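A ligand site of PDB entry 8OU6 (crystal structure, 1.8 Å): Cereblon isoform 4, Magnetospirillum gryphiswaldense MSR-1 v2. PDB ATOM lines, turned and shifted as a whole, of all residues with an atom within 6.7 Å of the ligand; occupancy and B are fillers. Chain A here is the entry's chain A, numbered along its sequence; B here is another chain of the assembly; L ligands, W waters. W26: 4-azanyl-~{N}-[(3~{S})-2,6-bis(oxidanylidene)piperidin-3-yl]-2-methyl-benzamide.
Water W1 lies within hydrogen-bond range of NE1 of Trp 81 and O3 of the ligand.
The side-chain hydroxyl (OH) of Tyr 83 sits at hydrogen-bond distance from an oxygen (O1) of the ligand (2.7 Å).
An oxygen (O3) of the ligand is in hydrogen-bond range of the side-chain amide nitrogen (ND2) of Asn 32, at 2.9 Å.
N of Trp 61 is in hydrogen-bond range of O1 of the ligand.
N1 of the ligand lies within hydrogen-bond range of O of Phe 59.
Merely in contact with the ligand: Trp 81 (3.4 Å), Ser 60 (3.4 Å), Pro 33 (3.5 Å) and Trp 67 (3.6 Å).
Hydrophobic or aromatic side chains that line the ligand: Pro 33, Phe 59, Trp 61, Trp 67, Trp 81 and Tyr 83.
Of the 19 residues printed, 8 come within 4 Å of the ligand.
Along chain A the residues within 4 Å of the ligand span positions 32 to 83.
The nearest printed residue that does not touch the ligand is Ala 34 (4.2 Å).
The backbone NH (N) of Met 36 sits at hydrogen-bond distance from the side-chain amide oxygen (OD1) of Asn 32, at 2.9 Å.
O of Tyr 65 sits at hydrogen-bond distance from OG of Ser 60, at 2.9 Å.
The side-chain hydroxyl of Ser 60 sits at hydrogen-bond distance from the backbone carbonyl oxygen of Phe 62 (3.0 Å).
The side-chain amide oxygen of Asn 32 lies within hydrogen-bond range of the backbone NH of Ala 34 (3.0 Å).
The backbone carbonyl oxygen of Phe 31 sits at hydrogen-bond distance from the indole nitrogen of Trp 61.
NE1 of Trp 67 lies within hydrogen-bond range of O of Glu 58 (2.8 Å).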
ATOM      1  N   VAL A  30       4.658  21.514  15.333  1.00  0.00           N
ATOM      2  CA  VAL A  30       4.031  21.614  14.015  1.00  0.00           C
ATOM      3  C   VAL A  30       5.064  21.214  12.973  1.00  0.00           C
ATOM      4  O   VAL A  30       6.266  21.244  13.241  1.00  0.00           O
ATOM      5  CB  VAL A  30       3.512  23.040  13.729  1.00  0.00           C
ATOM      6  CG1 VAL A  30       2.304  23.391  14.598  1.00  0.00           C
ATOM      7  CG2 VAL A  30       4.591  24.084  13.898  1.00  0.00           C
ATOM      8  N   PHE A  31       4.579  20.873  11.771  1.00  0.00           N
ATOM      9  CA  PHE A  31       5.472  20.573  10.674  1.00  0.00           C
ATOM     10  C   PHE A  31       5.012  21.327   9.447  1.00  0.00           C
ATOM     11  O   PHE A  31       3.823  21.546   9.236  1.00  0.00           O
ATOM     12  CB  PHE A  31       5.643  19.055  10.451  1.00  0.00           C
ATOM     13  CG  PHE A  31       4.516  18.326   9.774  1.00  0.00           C
ATOM     14  CD1 PHE A  31       4.540  18.139   8.395  1.00  0.00           C
ATOM     15  CD2 PHE A  31       3.542  17.685  10.512  1.00  0.00           C
ATOM     16  CE1 PHE A  31       3.557  17.394   7.756  1.00  0.00           C
ATOM     17  CE2 PHE A  31       2.541  16.953   9.874  1.00  0.00           C
ATOM     18  CZ  PHE A  31       2.562  16.808   8.491  1.00  0.00           C
ATOM     19  N   ASN A  32       5.993  21.772   8.665  1.00  0.00           N
ATOM     20  CA  ASN A  32       5.721  22.475   7.431  1.00  0.00           C
ATOM     21  C   ASN A  32       5.705  21.479   6.273  1.00  0.00           C
ATOM     22  O   ASN A  32       6.013  20.307   6.450  1.00  0.00           O
ATOM     23  CB  ASN A  32       6.682  23.660   7.296  1.00  0.00           C
ATOM     24  CG  ASN A  32       8.101  23.285   6.939  1.00  0.00           C
ATOM     25  OD1 ASN A  32       8.393  22.117   6.627  1.00  0.00           O
ATOM     26  ND2 ASN A  32       8.962  24.276   6.852  1.00  0.00           N
ATOM     27  N   PRO A  33       5.349  21.927   5.042  1.00  0.00           N
ATOM     28  CA  PRO A  33       5.304  21.030   3.893  1.00  0.00           C
ATOM     29  C   PRO A  33       6.661  20.532   3.409  1.00  0.00           C
ATOM     30  O   PRO A  33       6.710  19.629   2.590  1.00  0.00           O
ATOM     31  CB  PRO A  33       4.673  21.882   2.771  1.00  0.00           C
ATOM     32  CG  PRO A  33       4.093  23.107   3.464  1.00  0.00           C
ATOM     33  CD  PRO A  33       4.894  23.297   4.723  1.00  0.00           C
ATOM     34  N   ALA A  34       7.762  21.130   3.903  1.00  0.00           N
ATOM     35  CA  ALA A  34       9.108  20.666   3.647  1.00  0.00           C
ATOM     36  C   ALA A  34       9.522  19.597   4.657  1.00  0.00           C
ATOM     37  O   ALA A  34      10.652  19.141   4.649  1.00  0.00           O
ATOM     38  CB  ALA A  34      10.058  21.833   3.630  1.00  0.00           C
ATOM     39  N   MET A  36       9.842  19.914   7.916  1.00  0.00           N
ATOM     40  CA  MET A  36      10.565  20.389   9.081  1.00  0.00           C
ATOM     41  C   MET A  36       9.586  20.469  10.244  1.00  0.00           C
ATOM     42  O   MET A  36       8.478  20.969  10.081  1.00  0.00           O
ATOM     43  CB  MET A  36      11.164  21.756   8.790  1.00  0.00           C
ATOM     44  CG  MET A  36      12.021  21.785   7.582  1.00  0.00           C
ATOM     45  SD  MET A  36      12.510  23.456   7.116  1.00  0.00           S
ATOM     46  CE  MET A  36      13.579  23.070   5.723  1.00  0.00           C
ATOM     47  N   PHE A  38       8.828  21.963  14.047  1.00  0.00           N
ATOM     48  CA  PHE A  38       9.202  23.096  14.881  1.00  0.00           C
ATOM     49  C   PHE A  38       8.427  22.989  16.176  1.00  0.00           C
ATOM     50  O   PHE A  38       7.241  22.669  16.149  1.00  0.00           O
ATOM     51  CB  PHE A  38       8.856  24.428  14.211  1.00  0.00           C
ATOM     52  CG  PHE A  38       9.460  24.682  12.854  1.00  0.00           C
ATOM     53  CD1 PHE A  38      10.741  25.207  12.730  1.00  0.00           C
ATOM     54  CD2 PHE A  38       8.762  24.387  11.707  1.00  0.00           C
ATOM     55  CE1 PHE A  38      11.290  25.445  11.475  1.00  0.00           C
ATOM     56  CE2 PHE A  38       9.294  24.660  10.462  1.00  0.00           C
ATOM     57  CZ  PHE A  38      10.558  25.193  10.352  1.00  0.00           C
ATOM     58  N   GLU A  58      -1.517  30.521   3.323  1.00  0.00           N
ATOM     59  CA  GLU A  58      -1.215  29.186   2.816  1.00  0.00           C
ATOM     60  C   GLU A  58      -0.486  28.351   3.880  1.00  0.00           C
ATOM     61  O   GLU A  58       0.530  28.774   4.406  1.00  0.00           O
ATOM     62  CB  GLU A  58      -0.461  29.296   1.486  1.00  0.00           C
ATOM     63  CG  GLU A  58       0.921  29.927   1.578  1.00  0.00           C
ATOM     64  CD  GLU A  58       1.311  30.861   0.434  1.00  0.00           C
ATOM     65  OE1 GLU A  58       0.526  30.924  -0.546  1.00  0.00           O
ATOM     66  OE2 GLU A  58       2.376  31.548   0.535  1.00  0.00           O
ATOM     67  N   PHE A  59      -1.068  27.197   4.242  1.00  0.00           N
ATOM     68  CA  PHE A  59      -0.505  26.247   5.187  1.00  0.00           C
ATOM     69  C   PHE A  59      -0.404  26.816   6.601  1.00  0.00           C
ATOM     70  O   PHE A  59       0.393  26.312   7.425  1.00  0.00           O
ATOM     71  CB  PHE A  59       0.894  25.799   4.752  1.00  0.00           C
ATOM     72  CG  PHE A  59       0.958  25.215   3.358  1.00  0.00           C
ATOM     73  CD1 PHE A  59       0.302  24.020   3.076  1.00  0.00           C
ATOM     74  CD2 PHE A  59       1.619  25.872   2.328  1.00  0.00           C
ATOM     75  CE1 PHE A  59       0.333  23.486   1.795  1.00  0.00           C
ATOM     76  CE2 PHE A  59       1.627  25.345   1.053  1.00  0.00           C
ATOM     77  CZ  PHE A  59       0.984  24.152   0.786  1.00  0.00           C
ATOM     78  N   SER A  60      -1.181  27.858   6.922  1.00  0.00           N
ATOM     79  CA  SER A  60      -1.131  28.404   8.277  1.00  0.00           C
ATOM     80  C   SER A  60      -1.484  27.333   9.291  1.00  0.00           C
ATOM     81  O   SER A  60      -2.508  26.673   9.151  1.00  0.00           O
ATOM     82  CB  SER A  60      -2.026  29.609   8.435  1.00  0.00           C
ATOM     83  OG  SER A  60      -1.943  30.086   9.786  1.00  0.00           O
ATOM     84  N   TRP A  61      -0.679  27.179  10.361  1.00  0.00           N
ATOM     85  CA  TRP A  61      -0.983  26.244  11.432  1.00  0.00           C
ATOM     86  C   TRP A  61      -2.102  26.718  12.338  1.00  0.00           C
ATOM     87  O   TRP A  61      -2.550  25.978  13.226  1.00  0.00           O
ATOM     88  CB  TRP A  61       0.245  25.988  12.302  1.00  0.00           C
ATOM     89  CG  TRP A  61       1.348  25.333  11.541  1.00  0.00           C
ATOM     90  CD1 TRP A  61       1.270  24.165  10.804  1.00  0.00           C
ATOM     91  CD2 TRP A  61       2.693  25.787  11.440  1.00  0.00           C
ATOM     92  NE1 TRP A  61       2.489  23.885  10.233  1.00  0.00           N
ATOM     93  CE2 TRP A  61       3.385  24.844  10.635  1.00  0.00           C
ATOM     94  CE3 TRP A  61       3.395  26.911  11.918  1.00  0.00           C
ATOM     95  CZ2 TRP A  61       4.727  25.014  10.302  1.00  0.00           C
ATOM     96  CZ3 TRP A  61       4.737  27.041  11.629  1.00  0.00           C
ATOM     97  CH2 TRP A  61       5.395  26.096  10.828  1.00  0.00           C
ATOM     98  N   PHE A  62      -2.445  27.994  12.229  1.00  0.00           N
ATOM     99  CA  PHE A  62      -3.370  28.617  13.133  1.00  0.00           C
ATOM    100  C   PHE A  62      -4.544  29.125  12.325  1.00  0.00           C
ATOM    101  O   PHE A  62      -4.417  30.074  11.548  1.00  0.00           O
ATOM    102  CB  PHE A  62      -2.660  29.745  13.894  1.00  0.00           C
ATOM    103  CG  PHE A  62      -1.545  29.261  14.775  1.00  0.00           C
ATOM    104  CD1 PHE A  62      -1.811  28.676  15.986  1.00  0.00           C
ATOM    105  CD2 PHE A  62      -0.231  29.393  14.365  1.00  0.00           C
ATOM    106  CE1 PHE A  62      -0.779  28.230  16.801  1.00  0.00           C
ATOM    107  CE2 PHE A  62       0.800  28.925  15.170  1.00  0.00           C
ATOM    108  CZ  PHE A  62       0.530  28.333  16.386  1.00  0.00           C
ATOM    109  N   TYR A  65      -5.585  32.811  10.759  1.00  0.00           N
ATOM    110  CA  TYR A  65      -4.471  33.740  10.730  1.00  0.00           C
ATOM    111  C   TYR A  65      -3.642  33.576   9.469  1.00  0.00           C
ATOM    112  O   TYR A  65      -3.409  32.475   8.999  1.00  0.00           O
ATOM    113  CB  TYR A  65      -3.570  33.534  11.936  1.00  0.00           C
ATOM    114  CG  TYR A  65      -4.227  33.813  13.246  1.00  0.00           C
ATOM    115  CD1 TYR A  65      -4.233  35.084  13.775  1.00  0.00           C
ATOM    116  CD2 TYR A  65      -4.881  32.812  13.938  1.00  0.00           C
ATOM    117  CE1 TYR A  65      -4.842  35.372  14.989  1.00  0.00           C
ATOM    118  CE2 TYR A  65      -5.537  33.074  15.130  1.00  0.00           C
ATOM    119  CZ  TYR A  65      -5.534  34.365  15.635  1.00  0.00           C
ATOM    120  OH  TYR A  65      -6.091  34.535  16.836  1.00  0.00           O
ATOM    121  N   TRP A  67       0.250  34.489   7.927  1.00  0.00           N
ATOM    122  CA  TRP A  67       1.586  34.598   8.505  1.00  0.00           C
ATOM    123  C   TRP A  67       2.499  35.442   7.617  1.00  0.00           C
ATOM    124  O   TRP A  67       2.364  35.498   6.376  1.00  0.00           O
ATOM    125  CB  TRP A  67       2.175  33.209   8.753  1.00  0.00           C
ATOM    126  CG  TRP A  67       2.170  32.324   7.542  1.00  0.00           C
ATOM    127  CD1 TRP A  67       1.234  31.383   7.223  1.00  0.00           C
ATOM    128  CD2 TRP A  67       3.136  32.308   6.472  1.00  0.00           C
ATOM    129  NE1 TRP A  67       1.516  30.837   6.008  1.00  0.00           N
ATOM    130  CE2 TRP A  67       2.656  31.398   5.511  1.00  0.00           C
ATOM    131  CE3 TRP A  67       4.283  33.058   6.178  1.00  0.00           C
ATOM    132  CZ2 TRP A  67       3.369  31.108   4.353  1.00  0.00           C
ATOM    133  CZ3 TRP A  67       4.949  32.819   4.987  1.00  0.00           C
ATOM    134  CH2 TRP A  67       4.503  31.839   4.099  1.00  0.00           C
ATOM    135  N   ILE A  69       6.918  35.965   7.508  1.00  0.00           N
ATOM    136  CA  ILE A  69       8.197  35.481   8.025  1.00  0.00           C
ATOM    137  C   ILE A  69       8.802  36.551   8.936  1.00  0.00           C
ATOM    138  O   ILE A  69       8.798  37.738   8.604  1.00  0.00           O
ATOM    139  CB  ILE A  69       9.129  35.120   6.864  1.00  0.00           C
ATOM    140  CG1 ILE A  69       8.581  33.903   6.098  1.00  0.00           C
ATOM    141  CG2 ILE A  69      10.543  34.871   7.363  1.00  0.00           C
ATOM    142  CD1 ILE A  69       9.160  33.754   4.717  1.00  0.00           C
ATOM    143  N   HIS A  78      16.155  33.186  10.810  1.00  0.00           N
ATOM    144  CA  HIS A  78      14.706  32.999  10.788  1.00  0.00           C
ATOM    145  C   HIS A  78      14.220  32.563  12.164  1.00  0.00           C
ATOM    146  O   HIS A  78      14.546  31.478  12.590  1.00  0.00           O
ATOM    147  CB  HIS A  78      14.328  31.941   9.761  1.00  0.00           C
ATOM    148  CG  HIS A  78      12.867  31.660   9.737  1.00  0.00           C
ATOM    149  ND1 HIS A  78      12.366  30.438   9.354  1.00  0.00           N
ATOM    150  CD2 HIS A  78      11.827  32.461   9.947  1.00  0.00           C
ATOM    151  CE1 HIS A  78      11.040  30.497   9.376  1.00  0.00           C
ATOM    152  NE2 HIS A  78      10.684  31.729   9.732  1.00  0.00           N
ATOM    153  N   TRP A  81       7.379  33.400  12.795  1.00  0.00           N
ATOM    154  CA  TRP A  81       6.362  34.104  11.995  1.00  0.00           C
ATOM    155  C   TRP A  81       5.543  35.044  12.868  1.00  0.00           C
ATOM    156  O   TRP A  81       5.335  34.795  14.046  1.00  0.00           O
ATOM    157  CB  TRP A  81       5.441  33.070  11.334  1.00  0.00           C
ATOM    158  CG  TRP A  81       6.190  32.021  10.576  1.00  0.00           C
ATOM    159  CD1 TRP A  81       6.496  32.043   9.243  1.00  0.00           C
ATOM    160  CD2 TRP A  81       6.795  30.823  11.113  1.00  0.00           C
ATOM    161  NE1 TRP A  81       7.231  30.940   8.916  1.00  0.00           N
ATOM    162  CE2 TRP A  81       7.420  30.178  10.030  1.00  0.00           C
ATOM    163  CE3 TRP A  81       6.842  30.229  12.376  1.00  0.00           C
ATOM    164  CZ2 TRP A  81       8.111  28.981  10.189  1.00  0.00           C
ATOM    165  CZ3 TRP A  81       7.544  29.054  12.536  1.00  0.00           C
ATOM    166  CH2 TRP A  81       8.161  28.435  11.444  1.00  0.00           C
ATOM    167  N   TYR A  83       1.706  36.395  13.023  1.00  0.00           N
ATOM    168  CA  TYR A  83       0.387  35.992  12.566  1.00  0.00           C
ATOM    169  C   TYR A  83      -0.524  37.206  12.684  1.00  0.00           C
ATOM    170  O   TYR A  83      -0.457  37.914  13.696  1.00  0.00           O
ATOM    171  CB  TYR A  83      -0.121  34.830  13.409  1.00  0.00           C
ATOM    172  CG  TYR A  83       0.592  33.552  13.059  1.00  0.00           C
ATOM    173  CD1 TYR A  83       0.230  32.788  11.961  1.00  0.00           C
ATOM    174  CD2 TYR A  83       1.737  33.176  13.766  1.00  0.00           C
ATOM    175  CE1 TYR A  83       0.905  31.617  11.641  1.00  0.00           C
ATOM    176  CE2 TYR A  83       2.417  32.012  13.441  1.00  0.00           C
ATOM    177  CZ  TYR A  83       1.997  31.227  12.396  1.00  0.00           C
ATOM    178  OH  TYR A  83       2.720  30.093  12.056  1.00  0.00           O
ATOM    179  N   PRO B 104       0.363  19.974   7.326  1.00  0.00           N
ATOM    180  CA  PRO B 104      -0.396  19.726   6.106  1.00  0.00           C
ATOM    181  C   PRO B 104      -0.287  18.301   5.526  1.00  0.00           C
ATOM    182  O   PRO B 104       0.625  17.546   5.853  1.00  0.00           O
ATOM    183  CB  PRO B 104       0.219  20.732   5.116  1.00  0.00           C
ATOM    184  CG  PRO B 104       1.642  20.904   5.611  1.00  0.00           C
ATOM    185  CD  PRO B 104       1.522  20.854   7.121  1.00  0.00           C
HETATM  186  O2  W26 L   1       3.798  25.675   7.070  1.00  0.00           O
HETATM  187  O1  W26 L   1       1.881  28.718   9.844  1.00  0.00           O
HETATM  188  C1  W26 L   1       5.025  27.708   7.362  1.00  0.00           C
HETATM  189  C2  W26 L   1       4.680  29.182   7.555  1.00  0.00           C
HETATM  190  C3  W26 L   1       3.965  29.365   8.874  1.00  0.00           C
HETATM  191  C4  W26 L   1       2.781  28.467   9.050  1.00  0.00           C
HETATM  192  N1  W26 L   1       2.810  27.255   8.374  1.00  0.00           N
HETATM  193  C5  W26 L   1       3.841  26.785   7.582  1.00  0.00           C
HETATM  194  N2  W26 L   1       5.515  27.549   6.018  1.00  0.00           N
HETATM  195  C6  W26 L   1       6.721  27.020   5.772  1.00  0.00           C
HETATM  196  C7  W26 L   1       7.069  26.624   4.360  1.00  0.00           C
HETATM  197  C8  W26 L   1       8.375  26.149   4.166  1.00  0.00           C
HETATM  198  C9  W26 L   1       8.802  25.753   2.924  1.00  0.00           C
HETATM  199  C10 W26 L   1       7.949  25.809   1.831  1.00  0.00           C
HETATM  200  C11 W26 L   1       6.649  26.277   2.021  1.00  0.00           C
HETATM  201  C12 W26 L   1       6.191  26.692   3.260  1.00  0.00           C
HETATM  202  C13 W26 L   1       4.764  27.171   3.345  1.00  0.00           C
HETATM  203  N3  W26 L   1       8.376  25.413   0.589  1.00  0.00           N
HETATM  204  O3  W26 L   1       7.489  26.786   6.700  1.00  0.00           O
HETATM  205  O   HOH W   1       8.464  29.992   6.542  1.00  0.00           O
